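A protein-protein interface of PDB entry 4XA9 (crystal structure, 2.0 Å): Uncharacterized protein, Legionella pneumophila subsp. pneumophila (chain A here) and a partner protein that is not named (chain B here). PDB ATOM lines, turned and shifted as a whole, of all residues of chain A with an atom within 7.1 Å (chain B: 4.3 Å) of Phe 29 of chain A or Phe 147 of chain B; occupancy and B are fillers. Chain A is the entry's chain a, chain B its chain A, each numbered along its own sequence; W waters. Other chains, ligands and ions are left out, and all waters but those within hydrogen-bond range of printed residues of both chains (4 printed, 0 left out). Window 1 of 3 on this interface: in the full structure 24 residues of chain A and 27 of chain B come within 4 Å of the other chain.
NZ of Lys 195 of chain B is in salt-bridge range of OE2 of Glu 101 of chain A, at 3.7 Å. The side-chain hydroxyl (OG) of Ser 170 of chain B lies within hydrogen-bond range of the backbone carbonyl oxygen (O) of Asn 28 of chain A, 2.8 Å away. SG of Cys 102 of chain A sits at hydrogen-bond distance from NZ of Lys 195 of chain B (3.3 Å). O of His 132 of chain A lies within hydrogen-bond range of OH of Tyr 124 of chain B (2.8 Å).
The backbone NH of Tyr 124 of chain B lies within hydrogen-bond range of the backbone carbonyl oxygen of Cys 146 of chain B, at 2.9 Å. O of Cys 146 of chain B sits at hydrogen-bond distance from ND2 of Asn 148 of chain B (3.3 Å). The side-chain amide nitrogen (ND2) of Asn 148 of chain B lies close to the backbone NH (N) of Tyr 124 of chain B (3.3 Å). The backbone carbonyl oxygen (O) of Leu 138 of chain A is in hydrogen-bond range of the side-chain sulfur (SG) of Cys 102 of chain A. The side-chain sulfur (SG) of Cys 32 of chain A is in hydrogen-bond range of the side-chain hydroxyl (OH) of Tyr 194 of chain A (3.6 Å). The backbone NH (N) of Phe 147 of chain B lies within hydrogen-bond range of the backbone carbonyl oxygen (O) of Ser 170 of chain B, 3.0 Å away.
Asn 28 of chain A touches Cys 146 of chain B. Phe 29 of chain A touches Phe 147 of chain B (CD1 to CZ, 3.4 Å). CE1 of Phe 29 of chain A touches CB of Ser 170 of chain B, at 3.4 Å. Leu 123 of chain B touches His 31 of chain A (CD1 to CD2, 3.7 Å). Phe 147 of chain B touches Cys 32 of chain A (CE2 to SG, 3.8 Å). CG of Met 131 of chain A touches CE1 of Tyr 124 of chain B, 3.5 Å away. Phe 147 of chain B touches Met 131 of chain A. Phe 147 of chain B touches Ser 133 of chain A (O to OG, 3.7 Å). N of Ser 149 of chain B touches OG of Ser 133 of chain A (3.6 Å). Leu 138 of chain A touches Phe 147 of chain B.
Printed residues of chain B within 4 Å of Phe 29 of chain A: Phe 147 (3.4 Å) and Ser 170 (3.4 Å). Of chain A, only Phe 29, Cys 32, Met 131, Ser 133 and Leu 138 come within 4 Å of Phe 147 of chain B. Of the printed residues of chain B, Cys 32 of chain A touches Phe 147 (3.8 Å). Printed residues of chain B within 4 Å of His 132 of chain A: Tyr 124. Of the printed residues of chain B, Ser 133 of chain A touches Phe 147 (3.7 Å) and Ser 149 (3.6 Å). The nearest residue of chain A that does not touch Phe 147 of chain B is Trp 173 of chain A (4.9 Å). The nearest printed residue of chain A that does not touch Ser 149 of chain B is Leu 138 of chain A (6.8 Å).
Of the 11 printed residues of chain B, 7 touch a printed residue of chain A. Printed residues of chain B that touch a printed residue of chain A: Leu 123, Tyr 124, Cys 146, Phe 147, Ser 149, Ser 170 and Lys 195. Hydrophobic or aromatic side chains of chain B within 4 Å of the printed part of chain A: Leu 123, Tyr 124 and Phe 147.
Water W3 lies within hydrogen-bond range of the side-chain carboxylate (OD2) of Asp 25 of chain A, the side-chain amino group (NZ) of Lys 195 of chain B and the side-chain sulfur (SG) of Cys 102 of chain A. Water W2 lies within hydrogen-bond range of the side-chain hydroxyl of Ser 133 of chain A (2.7 Å), the backbone carbonyl oxygen of Ala 171 of chain B (2.9 Å) and the backbone NH of Ser 149 of chain B (3.2 Å). Water W1 lies within hydrogen-bond range of N of His 132 of chain A, OH of Tyr 124 of chain B and N of Met 131 of chain A. Water W4 bridges the backbone NH of His 31 of chain A (3.0 Å) and the side-chain sulfur of Cys 146 of chain B (3.4 Å).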
ATOM      1  N   ALA A  24      17.582  12.615  21.643  1.00  0.00           N
ATOM      2  CA  ALA A  24      18.362  13.836  21.483  1.00  0.00           C
ATOM      3  C   ALA A  24      17.650  14.925  20.680  1.00  0.00           C
ATOM      4  O   ALA A  24      17.925  16.108  20.886  1.00  0.00           O
ATOM      5  CB  ALA A  24      19.720  13.514  20.849  1.00  0.00           C
ATOM      6  N   ASP A  25      16.742  14.562  19.776  1.00  0.00           N
ATOM      7  CA  ASP A  25      16.096  15.606  18.976  1.00  0.00           C
ATOM      8  C   ASP A  25      14.766  16.075  19.571  1.00  0.00           C
ATOM      9  O   ASP A  25      13.937  16.642  18.872  1.00  0.00           O
ATOM     10  CB  ASP A  25      15.904  15.166  17.510  1.00  0.00           C
ATOM     11  CG  ASP A  25      15.206  13.829  17.366  1.00  0.00           C
ATOM     12  OD1 ASP A  25      14.762  13.259  18.380  1.00  0.00           O
ATOM     13  OD2 ASP A  25      15.099  13.348  16.215  1.00  0.00           O
ATOM     14  N   ILE A  26      14.581  15.866  20.871  1.00  0.00           N
ATOM     15  CA  ILE A  26      13.488  16.517  21.586  1.00  0.00           C
ATOM     16  C   ILE A  26      13.694  18.029  21.510  1.00  0.00           C
ATOM     17  O   ILE A  26      12.737  18.806  21.419  1.00  0.00           O
ATOM     18  CB  ILE A  26      13.414  16.028  23.043  1.00  0.00           C
ATOM     19  CG1 ILE A  26      12.773  14.633  23.069  1.00  0.00           C
ATOM     20  CG2 ILE A  26      12.656  17.028  23.927  1.00  0.00           C
ATOM     21  CD1 ILE A  26      12.717  13.989  24.425  1.00  0.00           C
ATOM     22  N   GLY A  27      14.961  18.438  21.495  1.00  0.00           N
ATOM     23  CA  GLY A  27      15.303  19.834  21.291  1.00  0.00           C
ATOM     24  C   GLY A  27      14.882  20.375  19.931  1.00  0.00           C
ATOM     25  O   GLY A  27      14.618  21.569  19.792  1.00  0.00           O
ATOM     26  N   ASN A  28      14.833  19.502  18.928  1.00  0.00           N
ATOM     27  CA  ASN A  28      14.403  19.885  17.583  1.00  0.00           C
ATOM     28  C   ASN A  28      12.881  19.838  17.440  1.00  0.00           C
ATOM     29  O   ASN A  28      12.264  20.726  16.843  1.00  0.00           O
ATOM     30  CB  ASN A  28      15.022  18.962  16.529  1.00  0.00           C
ATOM     31  CG  ASN A  28      16.540  19.057  16.466  1.00  0.00           C
ATOM     32  OD1 ASN A  28      17.127  20.072  16.831  1.00  0.00           O
ATOM     33  ND2 ASN A  28      17.179  17.987  15.989  1.00  0.00           N
ATOM     34  N   PHE A  29      12.285  18.781  17.983  1.00  0.00           N
ATOM     35  CA  PHE A  29      10.859  18.525  17.795  1.00  0.00           C
ATOM     36  C   PHE A  29      10.117  18.384  19.117  1.00  0.00           C
ATOM     37  O   PHE A  29       9.609  17.304  19.436  1.00  0.00           O
ATOM     38  CB  PHE A  29      10.658  17.269  16.948  1.00  0.00           C
ATOM     39  CG  PHE A  29      11.576  17.185  15.759  1.00  0.00           C
ATOM     40  CD1 PHE A  29      11.446  18.077  14.705  1.00  0.00           C
ATOM     41  CD2 PHE A  29      12.551  16.207  15.683  1.00  0.00           C
ATOM     42  CE1 PHE A  29      12.276  18.003  13.608  1.00  0.00           C
ATOM     43  CE2 PHE A  29      13.389  16.126  14.580  1.00  0.00           C
ATOM     44  CZ  PHE A  29      13.246  17.026  13.543  1.00  0.00           C
ATOM     45  N   PRO A  30      10.035  19.480  19.887  1.00  0.00           N
ATOM     46  CA  PRO A  30       9.421  19.401  21.218  1.00  0.00           C
ATOM     47  C   PRO A  30       7.962  18.953  21.157  1.00  0.00           C
ATOM     48  O   PRO A  30       7.501  18.262  22.067  1.00  0.00           O
ATOM     49  CB  PRO A  30       9.534  20.834  21.747  1.00  0.00           C
ATOM     50  CG  PRO A  30       9.615  21.676  20.535  1.00  0.00           C
ATOM     51  CD  PRO A  30      10.375  20.862  19.521  1.00  0.00           C
ATOM     52  N   HIS A  31       7.263  19.302  20.083  1.00  0.00           N
ATOM     53  CA  HIS A  31       5.847  18.980  19.982  1.00  0.00           C
ATOM     54  C   HIS A  31       5.596  17.518  19.616  1.00  0.00           C
ATOM     55  O   HIS A  31       4.447  17.096  19.535  1.00  0.00           O
ATOM     56  CB  HIS A  31       5.152  19.889  18.963  1.00  0.00           C
ATOM     57  CG  HIS A  31       3.675  20.006  19.176  1.00  0.00           C
ATOM     58  ND1 HIS A  31       3.130  20.367  20.390  1.00  0.00           N
ATOM     59  CD2 HIS A  31       2.629  19.818  18.334  1.00  0.00           C
ATOM     60  CE1 HIS A  31       1.812  20.396  20.287  1.00  0.00           C
ATOM     61  NE2 HIS A  31       1.482  20.067  19.050  1.00  0.00           N
ATOM     62  N   CYS A  32       6.658  16.741  19.411  1.00  0.00           N
ATOM     63  CA  CYS A  32       6.495  15.310  19.150  1.00  0.00           C
ATOM     64  C   CYS A  32       6.502  14.465  20.421  1.00  0.00           C
ATOM     65  O   CYS A  32       6.351  13.246  20.354  1.00  0.00           O
ATOM     66  CB  CYS A  32       7.579  14.811  18.196  1.00  0.00           C
ATOM     67  SG  CYS A  32       7.269  15.316  16.488  1.00  0.00           S
ATOM     68  N   LEU A  33       6.683  15.104  21.575  1.00  0.00           N
ATOM     69  CA  LEU A  33       6.583  14.395  22.844  1.00  0.00           C
ATOM     70  C   LEU A  33       5.140  13.968  23.056  1.00  0.00           C
ATOM     71  O   LEU A  33       4.221  14.772  22.909  1.00  0.00           O
ATOM     72  CB  LEU A  33       7.064  15.267  24.006  1.00  0.00           C
ATOM     73  CG  LEU A  33       8.568  15.335  24.260  1.00  0.00           C
ATOM     74  CD1 LEU A  33       8.870  16.403  25.295  1.00  0.00           C
ATOM     75  CD2 LEU A  33       9.082  13.985  24.740  1.00  0.00           C
ATOM     76  N   GLU A 101      18.166   9.335  18.034  1.00  0.00           N
ATOM     77  CA  GLU A 101      17.345  10.308  17.354  1.00  0.00           C
ATOM     78  C   GLU A 101      16.472   9.780  16.210  1.00  0.00           C
ATOM     79  O   GLU A 101      16.407   8.603  15.988  1.00  0.00           O
ATOM     80  CB  GLU A 101      17.983  11.666  17.167  1.00  0.00           C
ATOM     81  CG  GLU A 101      19.292  11.695  16.465  1.00  0.00           C
ATOM     82  CD  GLU A 101      19.177  11.133  15.108  1.00  0.00           C
ATOM     83  OE1 GLU A 101      19.316   9.930  14.978  1.00  0.00           O
ATOM     84  OE2 GLU A 101      18.948  11.915  14.193  1.00  0.00           O
ATOM     85  N   CYS A 102      15.749  10.645  15.547  1.00  0.00           N
ATOM     86  CA  CYS A 102      14.724  10.124  14.641  1.00  0.00           C
ATOM     87  C   CYS A 102      15.287   9.440  13.399  1.00  0.00           C
ATOM     88  O   CYS A 102      14.562   8.714  12.720  1.00  0.00           O
ATOM     89  CB  CYS A 102      13.758  11.233  14.213  1.00  0.00           C
ATOM     90  SG  CYS A 102      14.428  12.442  13.064  1.00  0.00           S
ATOM     91  N   MET A 131       7.846   9.776   6.506  1.00  0.00           N
ATOM     92  CA  MET A 131       7.554  11.193   6.696  1.00  0.00           C
ATOM     93  C   MET A 131       8.169  12.016   5.556  1.00  0.00           C
ATOM     94  O   MET A 131       9.087  12.812   5.756  1.00  0.00           O
ATOM     95  CB  MET A 131       8.062  11.675   8.063  1.00  0.00           C
ATOM     96  CG  MET A 131       7.364  12.925   8.582  1.00  0.00           C
ATOM     97  SD  MET A 131       7.899  13.413  10.389  1.00  0.00           S
ATOM     98  CE  MET A 131       7.363  11.825  11.384  1.00  0.00           C
ATOM     99  N   HIS A 132       7.658  11.794   4.352  1.00  0.00           N
ATOM    100  CA  HIS A 132       8.183  12.435   3.153  1.00  0.00           C
ATOM    101  C   HIS A 132       7.830  13.919   3.118  1.00  0.00           C
ATOM    102  O   HIS A 132       6.684  14.298   3.353  1.00  0.00           O
ATOM    103  CB  HIS A 132       7.647  11.727   1.902  1.00  0.00           C
ATOM    104  CG  HIS A 132       7.947  12.444   0.622  1.00  0.00           C
ATOM    105  ND1 HIS A 132       7.042  13.285   0.008  1.00  0.00           N
ATOM    106  CD2 HIS A 132       9.056  12.456  -0.154  1.00  0.00           C
ATOM    107  CE1 HIS A 132       7.579  13.777  -1.095  1.00  0.00           C
ATOM    108  NE2 HIS A 132       8.801  13.290  -1.214  1.00  0.00           N
ATOM    109  N   SER A 133       8.829  14.757   2.843  1.00  0.00           N
ATOM    110  CA  SER A 133       8.610  16.186   2.679  1.00  0.00           C
ATOM    111  C   SER A 133       9.513  16.750   1.587  1.00  0.00           C
ATOM    112  O   SER A 133      10.720  16.908   1.790  1.00  0.00           O
ATOM    113  CB  SER A 133       8.849  16.933   3.995  1.00  0.00           C
ATOM    114  OG  SER A 133       8.604  18.322   3.835  1.00  0.00           O
ATOM    115  N   LEU A 138      12.106  12.304   6.438  1.00  0.00           N
ATOM    116  CA  LEU A 138      12.583  12.879   7.688  1.00  0.00           C
ATOM    117  C   LEU A 138      12.621  11.897   8.857  1.00  0.00           C
ATOM    118  O   LEU A 138      13.173  12.204   9.911  1.00  0.00           O
ATOM    119  CB  LEU A 138      11.704  14.084   8.049  1.00  0.00           C
ATOM    120  CG  LEU A 138      11.438  15.048   6.888  1.00  0.00           C
ATOM    121  CD1 LEU A 138      10.387  16.087   7.245  1.00  0.00           C
ATOM    122  CD2 LEU A 138      12.730  15.732   6.469  1.00  0.00           C
ATOM    123  N   HIS A 139      12.053  10.713   8.665  1.00  0.00           N
ATOM    124  CA  HIS A 139      11.838   9.789   9.775  1.00  0.00           C
ATOM    125  C   HIS A 139      12.110   8.347   9.357  1.00  0.00           C
ATOM    126  O   HIS A 139      11.457   7.826   8.461  1.00  0.00           O
ATOM    127  CB  HIS A 139      10.404   9.942  10.280  1.00  0.00           C
ATOM    128  CG  HIS A 139      10.034   9.006  11.386  1.00  0.00           C
ATOM    129  ND1 HIS A 139       8.747   8.550  11.562  1.00  0.00           N
ATOM    130  CD2 HIS A 139      10.768   8.463  12.387  1.00  0.00           C
ATOM    131  CE1 HIS A 139       8.705   7.751  12.614  1.00  0.00           C
ATOM    132  NE2 HIS A 139       9.917   7.679  13.132  1.00  0.00           N
ATOM    133  N   TRP A 173      11.684   5.289  18.087  1.00  0.00           N
ATOM    134  CA  TRP A 173      11.728   6.732  18.307  1.00  0.00           C
ATOM    135  C   TRP A 173      10.400   7.201  18.891  1.00  0.00           C
ATOM    136  O   TRP A 173      10.365   8.007  19.819  1.00  0.00           O
ATOM    137  CB  TRP A 173      12.035   7.463  17.001  1.00  0.00           C
ATOM    138  CG  TRP A 173      12.086   8.959  17.114  1.00  0.00           C
ATOM    139  CD1 TRP A 173      13.098   9.712  17.632  1.00  0.00           C
ATOM    140  CD2 TRP A 173      11.087   9.882  16.669  1.00  0.00           C
ATOM    141  NE1 TRP A 173      12.788  11.049  17.542  1.00  0.00           N
ATOM    142  CE2 TRP A 173      11.558  11.179  16.953  1.00  0.00           C
ATOM    143  CE3 TRP A 173       9.837   9.736  16.055  1.00  0.00           C
ATOM    144  CZ2 TRP A 173      10.822  12.323  16.650  1.00  0.00           C
ATOM    145  CZ3 TRP A 173       9.106  10.875  15.757  1.00  0.00           C
ATOM    146  CH2 TRP A 173       9.600  12.152  16.056  1.00  0.00           C
ATOM    147  N   MET A 177       9.685   8.892  22.436  1.00  0.00           N
ATOM    148  CA  MET A 177       8.884  10.108  22.577  1.00  0.00           C
ATOM    149  C   MET A 177       7.682   9.916  23.511  1.00  0.00           C
ATOM    150  O   MET A 177       7.012  10.883  23.879  1.00  0.00           O
ATOM    151  CB  MET A 177       8.405  10.580  21.205  1.00  0.00           C
ATOM    152  CG  MET A 177       9.467  11.286  20.376  1.00  0.00           C
ATOM    153  SD  MET A 177      10.173  12.881  21.275  1.00  0.00           S
ATOM    154  CE  MET A 177      11.155  13.672  19.783  1.00  0.00           C
ATOM    155  N   TYR A 194       2.393   6.953  13.894  1.00  0.00           N
ATOM    156  CA  TYR A 194       2.702   7.871  12.799  1.00  0.00           C
ATOM    157  C   TYR A 194       2.206   7.360  11.460  1.00  0.00           C
ATOM    158  O   TYR A 194       2.791   7.634  10.409  1.00  0.00           O
ATOM    159  CB  TYR A 194       4.208   8.165  12.755  1.00  0.00           C
ATOM    160  CG  TYR A 194       4.564   9.241  13.747  1.00  0.00           C
ATOM    161  CD1 TYR A 194       4.796   8.932  15.084  1.00  0.00           C
ATOM    162  CD2 TYR A 194       4.603  10.575  13.366  1.00  0.00           C
ATOM    163  CE1 TYR A 194       5.085   9.917  16.005  1.00  0.00           C
ATOM    164  CE2 TYR A 194       4.892  11.570  14.282  1.00  0.00           C
ATOM    165  CZ  TYR A 194       5.129  11.234  15.598  1.00  0.00           C
ATOM    166  OH  TYR A 194       5.421  12.223  16.507  1.00  0.00           O
ATOM    167  N   LEU B 123       2.548  20.965  12.314  1.00  0.00           N
ATOM    168  CA  LEU B 123       3.653  20.130  11.856  1.00  0.00           C
ATOM    169  C   LEU B 123       3.189  19.223  10.728  1.00  0.00           C
ATOM    170  O   LEU B 123       2.045  18.760  10.734  1.00  0.00           O
ATOM    171  CB  LEU B 123       4.208  19.276  13.002  1.00  0.00           C
ATOM    172  CG  LEU B 123       4.961  19.921  14.165  1.00  0.00           C
ATOM    173  CD1 LEU B 123       4.018  20.712  15.066  1.00  0.00           C
ATOM    174  CD2 LEU B 123       5.672  18.846  14.976  1.00  0.00           C
ATOM    175  N   TYR B 124       4.091  18.963   9.784  1.00  0.00           N
ATOM    176  CA  TYR B 124       3.857  18.033   8.670  1.00  0.00           C
ATOM    177  C   TYR B 124       2.485  18.188   8.010  1.00  0.00           C
ATOM    178  O   TYR B 124       1.591  17.379   8.224  1.00  0.00           O
ATOM    179  CB  TYR B 124       4.038  16.582   9.137  1.00  0.00           C
ATOM    180  CG  TYR B 124       4.206  15.618   7.983  1.00  0.00           C
ATOM    181  CD1 TYR B 124       5.397  15.573   7.267  1.00  0.00           C
ATOM    182  CD2 TYR B 124       3.173  14.768   7.596  1.00  0.00           C
ATOM    183  CE1 TYR B 124       5.560  14.707   6.199  1.00  0.00           C
ATOM    184  CE2 TYR B 124       3.326  13.894   6.527  1.00  0.00           C
ATOM    185  CZ  TYR B 124       4.523  13.871   5.834  1.00  0.00           C
ATOM    186  OH  TYR B 124       4.692  13.010   4.770  1.00  0.00           O
ATOM    187  N   LEU B 145       5.997  24.722  12.884  1.00  0.00           N
ATOM    188  CA  LEU B 145       5.882  24.290  11.495  1.00  0.00           C
ATOM    189  C   LEU B 145       6.847  23.167  11.116  1.00  0.00           C
ATOM    190  O   LEU B 145       7.181  23.015   9.943  1.00  0.00           O
ATOM    191  CB  LEU B 145       6.110  25.483  10.558  1.00  0.00           C
ATOM    192  CG  LEU B 145       5.031  26.557  10.621  1.00  0.00           C
ATOM    193  CD1 LEU B 145       5.441  27.805   9.844  1.00  0.00           C
ATOM    194  CD2 LEU B 145       3.711  25.986  10.098  1.00  0.00           C
ATOM    195  N   CYS B 146       7.288  22.384  12.096  1.00  0.00           N
ATOM    196  CA  CYS B 146       8.249  21.309  11.840  1.00  0.00           C
ATOM    197  C   CYS B 146       7.771  20.379  10.730  1.00  0.00           C
ATOM    198  O   CYS B 146       6.576  20.145  10.595  1.00  0.00           O
ATOM    199  CB  CYS B 146       8.507  20.497  13.109  1.00  0.00           C
ATOM    200  SG  CYS B 146       9.283  21.433  14.430  1.00  0.00           S
ATOM    201  N   PHE B 147       8.714  19.874   9.938  1.00  0.00           N
ATOM    202  CA  PHE B 147       8.440  18.906   8.871  1.00  0.00           C
ATOM    203  C   PHE B 147       7.606  19.491   7.739  1.00  0.00           C
ATOM    204  O   PHE B 147       6.876  18.765   7.067  1.00  0.00           O
ATOM    205  CB  PHE B 147       7.735  17.652   9.414  1.00  0.00           C
ATOM    206  CG  PHE B 147       8.368  17.075  10.654  1.00  0.00           C
ATOM    207  CD1 PHE B 147       9.665  16.585  10.629  1.00  0.00           C
ATOM    208  CD2 PHE B 147       7.646  16.986  11.832  1.00  0.00           C
ATOM    209  CE1 PHE B 147      10.244  16.044  11.761  1.00  0.00           C
ATOM    210  CE2 PHE B 147       8.219  16.443  12.974  1.00  0.00           C
ATOM    211  CZ  PHE B 147       9.521  15.968  12.935  1.00  0.00           C
ATOM    212  N   ASN B 148       7.711  20.799   7.539  1.00  0.00           N
ATOM    213  CA  ASN B 148       7.139  21.464   6.368  1.00  0.00           C
ATOM    214  C   ASN B 148       8.256  22.117   5.559  1.00  0.00           C
ATOM    215  O   ASN B 148       9.062  22.864   6.109  1.00  0.00           O
ATOM    216  CB  ASN B 148       6.109  22.530   6.763  1.00  0.00           C
ATOM    217  CG  ASN B 148       4.852  21.939   7.378  1.00  0.00           C
ATOM    218  OD1 ASN B 148       3.992  21.405   6.674  1.00  0.00           O
ATOM    219  ND2 ASN B 148       4.728  22.054   8.697  1.00  0.00           N
ATOM    220  N   SER B 149       8.305  21.848   4.261  1.00  0.00           N
ATOM    221  CA  SER B 149       9.357  22.433   3.428  1.00  0.00           C
ATOM    222  C   SER B 149       9.095  23.919   3.190  1.00  0.00           C
ATOM    223  O   SER B 149       8.628  24.318   2.121  1.00  0.00           O
ATOM    224  CB  SER B 149       9.469  21.690   2.095  1.00  0.00           C
ATOM    225  OG  SER B 149      10.555  22.188   1.326  1.00  0.00           O
ATOM    226  N   SER B 170      11.744  23.188  12.632  1.00  0.00           N
ATOM    227  CA  SER B 170      12.799  22.198  12.439  1.00  0.00           C
ATOM    228  C   SER B 170      12.466  21.287  11.263  1.00  0.00           C
ATOM    229  O   SER B 170      11.301  20.968  11.042  1.00  0.00           O
ATOM    230  CB  SER B 170      13.004  21.362  13.710  1.00  0.00           C
ATOM    231  OG  SER B 170      13.448  22.159  14.800  1.00  0.00           O
ATOM    232  N   ALA B 171      13.494  20.860  10.533  1.00  0.00           N
ATOM    233  CA  ALA B 171      13.321  20.050   9.323  1.00  0.00           C
ATOM    234  C   ALA B 171      12.430  20.771   8.319  1.00  0.00           C
ATOM    235  O   ALA B 171      11.429  20.220   7.852  1.00  0.00           O
ATOM    236  CB  ALA B 171      12.746  18.674   9.665  1.00  0.00           C
ATOM    237  N   CYS B 172      12.795  22.009   7.997  1.00  0.00           N
ATOM    238  CA  CYS B 172      11.988  22.835   7.108  1.00  0.00           C
ATOM    239  C   CYS B 172      12.760  23.335   5.889  1.00  0.00           C
ATOM    240  O   CYS B 172      12.337  24.295   5.238  1.00  0.00           O
ATOM    241  CB  CYS B 172      11.408  24.030   7.875  1.00  0.00           C
ATOM    242  SG  CYS B 172      10.117  23.599   9.092  1.00  0.00           S
ATOM    243  N   LYS B 195      17.703  20.451  12.591  1.00  0.00           N
ATOM    244  CA  LYS B 195      17.572  19.524  11.390  1.00  0.00           C
ATOM    245  C   LYS B 195      17.438  20.275  10.040  1.00  0.00           C
ATOM    246  O   LYS B 195      16.584  19.945   9.210  1.00  0.00           O
ATOM    247  CB  LYS B 195      16.533  18.509  11.566  1.00  0.00           C
ATOM    248  CG  LYS B 195      16.692  17.197  10.872  1.00  0.00           C
ATOM    249  CD  LYS B 195      17.728  16.334  11.502  1.00  0.00           C
ATOM    250  CE  LYS B 195      17.709  14.961  10.896  1.00  0.00           C
ATOM    251  NZ  LYS B 195      17.080  14.025  11.853  1.00  0.00           N
HETATM  252  O   HOH W   1       5.647   9.955   3.933  1.00  0.00           O
HETATM  253  O   HOH W   2      10.560  19.685   5.150  1.00  0.00           O
HETATM  254  O   HOH W   3      16.626  14.631  14.446  1.00  0.00           O
HETATM  255  O   HOH W   4       7.903  20.708  17.463  1.00  0.00           O
